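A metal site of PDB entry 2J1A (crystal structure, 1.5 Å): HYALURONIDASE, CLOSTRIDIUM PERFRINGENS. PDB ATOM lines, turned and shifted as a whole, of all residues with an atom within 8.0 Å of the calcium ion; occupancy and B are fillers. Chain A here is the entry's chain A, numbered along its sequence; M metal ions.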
ATOM      1  N   PRO A  27      -7.287  24.739 -16.634  1.00  0.00           N
ATOM      2  CA  PRO A  27      -8.320  23.987 -17.356  1.00  0.00           C
ATOM      3  C   PRO A  27      -9.162  23.144 -16.387  1.00  0.00           C
ATOM      4  O   PRO A  27      -8.741  22.857 -15.242  1.00  0.00           O
ATOM      5  CB  PRO A  27      -7.513  23.034 -18.247  1.00  0.00           C
ATOM      6  CG  PRO A  27      -6.282  22.791 -17.464  1.00  0.00           C
ATOM      7  CD  PRO A  27      -5.941  24.186 -16.922  1.00  0.00           C
ATOM      8  N   ALA A  28     -10.338  22.717 -16.880  1.00  0.00           N
ATOM      9  CA  ALA A  28     -11.242  21.839 -16.094  1.00  0.00           C
ATOM     10  C   ALA A  28     -10.515  20.579 -15.586  1.00  0.00           C
ATOM     11  O   ALA A  28     -10.777  20.125 -14.473  1.00  0.00           O
ATOM     12  CB  ALA A  28     -12.480  21.484 -16.897  1.00  0.00           C
ATOM     13  N   SER A  29      -9.582  20.045 -16.409  1.00  0.00           N
ATOM     14  CA  SER A  29      -8.872  18.794 -16.052  1.00  0.00           C
ATOM     15  C   SER A  29      -8.099  18.978 -14.740  1.00  0.00           C
ATOM     16  O   SER A  29      -7.820  18.010 -14.036  1.00  0.00           O
ATOM     17  CB  SER A  29      -7.909  18.372 -17.171  1.00  0.00           C
ATOM     18  OG  SER A  29      -6.907  19.343 -17.381  1.00  0.00           O
ATOM     19  N   PHE A  30      -7.745  20.225 -14.414  1.00  0.00           N
ATOM     20  CA  PHE A  30      -7.031  20.498 -13.165  1.00  0.00           C
ATOM     21  C   PHE A  30      -7.894  20.240 -11.907  1.00  0.00           C
ATOM     22  O   PHE A  30      -7.345  20.166 -10.819  1.00  0.00           O
ATOM     23  CB  PHE A  30      -6.437  21.916 -13.170  1.00  0.00           C
ATOM     24  CG  PHE A  30      -5.078  22.029 -13.858  1.00  0.00           C
ATOM     25  CD1 PHE A  30      -4.576  21.006 -14.693  1.00  0.00           C
ATOM     26  CD2 PHE A  30      -4.318  23.184 -13.695  1.00  0.00           C
ATOM     27  CE1 PHE A  30      -3.332  21.115 -15.325  1.00  0.00           C
ATOM     28  CE2 PHE A  30      -3.066  23.315 -14.348  1.00  0.00           C
ATOM     29  CZ  PHE A  30      -2.586  22.272 -15.160  1.00  0.00           C
ATOM     30  N   ALA A  31      -9.214  20.139 -12.053  1.00  0.00           N
ATOM     31  CA  ALA A  31     -10.090  19.741 -10.953  1.00  0.00           C
ATOM     32  C   ALA A  31     -10.148  18.222 -10.696  1.00  0.00           C
ATOM     33  O   ALA A  31     -10.801  17.784  -9.741  1.00  0.00           O
ATOM     34  CB  ALA A  31     -11.543  20.324 -11.144  1.00  0.00           C
ATOM     35  N   SER A  32      -9.457  17.450 -11.541  1.00  0.00           N
ATOM     36  CA  SER A  32      -9.508  15.987 -11.565  1.00  0.00           C
ATOM     37  C   SER A  32      -8.118  15.332 -11.564  1.00  0.00           C
ATOM     38  O   SER A  32      -8.001  14.153 -11.909  1.00  0.00           O
ATOM     39  CB  SER A  32     -10.284  15.521 -12.815  1.00  0.00           C
ATOM     40  OG  SER A  32      -9.484  15.688 -14.000  1.00  0.00           O
ATOM     41  N   ASP A  33      -7.073  16.092 -11.199  1.00  0.00           N
ATOM     42  CA  ASP A  33      -5.684  15.584 -11.335  1.00  0.00           C
ATOM     43  C   ASP A  33      -5.032  15.156 -10.006  1.00  0.00           C
ATOM     44  O   ASP A  33      -3.808  14.956  -9.932  1.00  0.00           O
ATOM     45  CB  ASP A  33      -4.827  16.591 -12.118  1.00  0.00           C
ATOM     46  CG  ASP A  33      -4.583  17.884 -11.347  1.00  0.00           C
ATOM     47  OD1 ASP A  33      -3.903  18.783 -11.885  1.00  0.00           O
ATOM     48  OD2 ASP A  33      -5.045  17.978 -10.208  1.00  0.00           O
ATOM     49  N   GLY A  34      -5.839  15.036  -8.959  1.00  0.00           N
ATOM     50  CA  GLY A  34      -5.357  14.639  -7.631  1.00  0.00           C
ATOM     51  C   GLY A  34      -4.363  15.575  -6.932  1.00  0.00           C
ATOM     52  O   GLY A  34      -3.826  15.246  -5.871  1.00  0.00           O
ATOM     53  N   ASP A  35      -4.158  16.760  -7.502  1.00  0.00           N
ATOM     54  CA  ASP A  35      -3.152  17.720  -7.008  1.00  0.00           C
ATOM     55  C   ASP A  35      -3.821  18.975  -6.431  1.00  0.00           C
ATOM     56  O   ASP A  35      -4.481  19.710  -7.161  1.00  0.00           O
ATOM     57  CB  ASP A  35      -2.237  18.061  -8.197  1.00  0.00           C
ATOM     58  CG  ASP A  35      -1.038  18.920  -7.820  1.00  0.00           C
ATOM     59  OD1 ASP A  35      -1.004  19.504  -6.719  1.00  0.00           O
ATOM     60  OD2 ASP A  35      -0.116  19.015  -8.680  1.00  0.00           O
ATOM     61  N   MET A  36      -3.693  19.206  -5.135  1.00  0.00           N
ATOM     62  CA  MET A  36      -4.346  20.384  -4.504  1.00  0.00           C
ATOM     63  C   MET A  36      -3.764  21.744  -4.965  1.00  0.00           C
ATOM     64  O   MET A  36      -4.377  22.789  -4.699  1.00  0.00           O
ATOM     65  CB  MET A  36      -4.300  20.335  -2.975  1.00  0.00           C
ATOM     66  CG  MET A  36      -5.329  19.396  -2.374  1.00  0.00           C
ATOM     67  SD  MET A  36      -7.053  19.969  -2.679  1.00  0.00           S
ATOM     68  CE  MET A  36      -7.095  21.591  -1.874  1.00  0.00           C
ATOM     69  N   ASN A  37      -2.594  21.720  -5.614  1.00  0.00           N
ATOM     70  CA  ASN A  37      -1.912  22.957  -6.072  1.00  0.00           C
ATOM     71  C   ASN A  37      -2.347  23.421  -7.458  1.00  0.00           C
ATOM     72  O   ASN A  37      -1.862  24.440  -7.957  1.00  0.00           O
ATOM     73  CB  ASN A  37      -0.388  22.783  -6.033  1.00  0.00           C
ATOM     74  CG  ASN A  37       0.161  22.702  -4.607  1.00  0.00           C
ATOM     75  OD1 ASN A  37      -0.394  23.303  -3.667  1.00  0.00           O
ATOM     76  ND2 ASN A  37       1.265  21.979  -4.446  1.00  0.00           N
ATOM     77  N   THR A  38      -3.211  22.641  -8.101  1.00  0.00           N
ATOM     78  CA  THR A  38      -3.732  22.966  -9.403  1.00  0.00           C
ATOM     79  C   THR A  38      -5.262  23.102  -9.265  1.00  0.00           C
ATOM     80  O   THR A  38      -5.896  22.302  -8.576  1.00  0.00           O
ATOM     81  CB  THR A  38      -3.399  21.908 -10.495  1.00  0.00           C
ATOM     82  OG1 THR A  38      -4.050  20.672 -10.190  1.00  0.00           O
ATOM     83  CG2 THR A  38      -1.880  21.656 -10.644  1.00  0.00           C
ATOM     84  N   PHE A  39      -5.808  24.128  -9.891  1.00  0.00           N
ATOM     85  CA  PHE A  39      -7.242  24.365  -9.823  1.00  0.00           C
ATOM     86  C   PHE A  39      -7.786  24.660 -11.217  1.00  0.00           C
ATOM     87  O   PHE A  39      -7.059  25.160 -12.116  1.00  0.00           O
ATOM     88  CB  PHE A  39      -7.561  25.487  -8.850  1.00  0.00           C
ATOM     89  CG  PHE A  39      -6.849  26.772  -9.153  1.00  0.00           C
ATOM     90  CD1 PHE A  39      -7.408  27.689 -10.062  1.00  0.00           C
ATOM     91  CD2 PHE A  39      -5.628  27.090  -8.527  1.00  0.00           C
ATOM     92  CE1 PHE A  39      -6.771  28.887 -10.355  1.00  0.00           C
ATOM     93  CE2 PHE A  39      -4.975  28.294  -8.827  1.00  0.00           C
ATOM     94  CZ  PHE A  39      -5.562  29.189  -9.743  1.00  0.00           C
ATOM     95  N   TRP A  40      -9.046  24.276 -11.405  1.00  0.00           N
ATOM     96  CA  TRP A  40      -9.847  24.729 -12.530  1.00  0.00           C
ATOM     97  C   TRP A  40     -10.286  26.155 -12.169  1.00  0.00           C
ATOM     98  O   TRP A  40     -10.630  26.446 -11.005  1.00  0.00           O
ATOM     99  CB  TRP A  40     -11.083  23.830 -12.696  1.00  0.00           C
ATOM    100  CG  TRP A  40     -12.217  24.503 -13.464  1.00  0.00           C
ATOM    101  CD1 TRP A  40     -12.187  24.889 -14.780  1.00  0.00           C
ATOM    102  CD2 TRP A  40     -13.528  24.835 -12.977  1.00  0.00           C
ATOM    103  NE1 TRP A  40     -13.398  25.448 -15.151  1.00  0.00           N
ATOM    104  CE2 TRP A  40     -14.250  25.423 -14.055  1.00  0.00           C
ATOM    105  CE3 TRP A  40     -14.166  24.688 -11.732  1.00  0.00           C
ATOM    106  CZ2 TRP A  40     -15.573  25.872 -13.935  1.00  0.00           C
ATOM    107  CZ3 TRP A  40     -15.511  25.166 -11.603  1.00  0.00           C
ATOM    108  CH2 TRP A  40     -16.189  25.745 -12.713  1.00  0.00           C
ATOM    109  N   ALA A  71     -12.989  20.422  -3.031  1.00  0.00           N
ATOM    110  CA  ALA A  71     -11.847  21.051  -2.379  1.00  0.00           C
ATOM    111  C   ALA A  71     -11.590  22.456  -3.036  1.00  0.00           C
ATOM    112  O   ALA A  71     -11.257  22.572  -4.234  1.00  0.00           O
ATOM    113  CB  ALA A  71     -10.628  20.158  -2.499  1.00  0.00           C
ATOM    114  N   ALA A 143     -12.130  25.278  -8.492  1.00  0.00           N
ATOM    115  CA  ALA A 143     -12.054  24.065  -7.698  1.00  0.00           C
ATOM    116  C   ALA A 143     -10.644  23.497  -7.813  1.00  0.00           C
ATOM    117  O   ALA A 143     -10.157  23.291  -8.925  1.00  0.00           O
ATOM    118  CB  ALA A 143     -13.061  23.041  -8.211  1.00  0.00           C
ATOM    119  N   ALA A 144     -10.023  23.228  -6.673  1.00  0.00           N
ATOM    120  CA  ALA A 144      -8.724  22.530  -6.646  1.00  0.00           C
ATOM    121  C   ALA A 144      -8.936  21.058  -6.989  1.00  0.00           C
ATOM    122  O   ALA A 144      -8.220  20.511  -7.820  1.00  0.00           O
ATOM    123  CB  ALA A 144      -8.021  22.649  -5.278  1.00  0.00           C
ATOM    124  N   GLU A 145      -9.947  20.428  -6.387  1.00  0.00           N
ATOM    125  CA  GLU A 145     -10.277  19.044  -6.714  1.00  0.00           C
ATOM    126  C   GLU A 145     -11.773  18.820  -6.552  1.00  0.00           C
ATOM    127  O   GLU A 145     -12.404  19.408  -5.658  1.00  0.00           O
ATOM    128  CB  GLU A 145      -9.556  18.080  -5.747  1.00  0.00           C
ATOM    129  CG  GLU A 145      -8.053  17.976  -5.988  1.00  0.00           C
ATOM    130  CD  GLU A 145      -7.743  17.281  -7.259  1.00  0.00           C
ATOM    131  OE1 GLU A 145      -7.046  17.843  -8.106  1.00  0.00           O
ATOM    132  OE2 GLU A 145      -8.217  16.164  -7.459  1.00  0.00           O
ATOM    133  N   VAL A 146     -12.325  17.943  -7.394  1.00  0.00           N
ATOM    134  CA  VAL A 146     -13.724  17.524  -7.244  1.00  0.00           C
ATOM    135  C   VAL A 146     -13.707  16.066  -7.638  1.00  0.00           C
ATOM    136  O   VAL A 146     -13.133  15.698  -8.694  1.00  0.00           O
ATOM    137  CB  VAL A 146     -14.708  18.286  -8.186  1.00  0.00           C
ATOM    138  CG1 VAL A 146     -16.168  17.722  -8.051  1.00  0.00           C
ATOM    139  CG2 VAL A 146     -14.697  19.755  -7.900  1.00  0.00           C
HETATM  140 CA    CA M   1      -6.102  19.894  -8.849  1.00  0.00          CA
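OD1 of Asp 35 lies within hydrogen-bond range of N of Asn 37 (2.9 Å).
The side-chain carboxylate (OE2) of Glu 145 lies within hydrogen-bond range of the backbone NH (N) of Gly 34, 3.0 Å away.
O of Glu 145 is in hydrogen-bond range of N of Ala 71 (2.9 Å).
The backbone carbonyl oxygen (O) of Ala 71 is in hydrogen-bond range of the backbone NH (N) of Ala 144, 2.8 Å away.
Six residues have an atom within 4 Å of the calcium ion: Phe 30, Asp 33, Asp 35, Thr 38, Ala 144 and Glu 145.
The nearest printed residue that does not touch the calcium ion is Phe 39 (4.4 Å).
The calcium ion is bound by the backbone carbonyl oxygen of Phe 30 (2.3 Å), the backbone carbonyl oxygen of Asp 35 (2.3 Å), the side-chain carboxylate of Glu 145 (2.4 Å), the backbone carbonyl oxygen of Thr 38 (2.4 Å), the backbone carbonyl oxygen of Ala 144 (2.4 Å), the side-chain hydroxyl of Thr 38 (2.6 Å) and the side-chain carboxylate of Asp 33 (2.6 Å).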
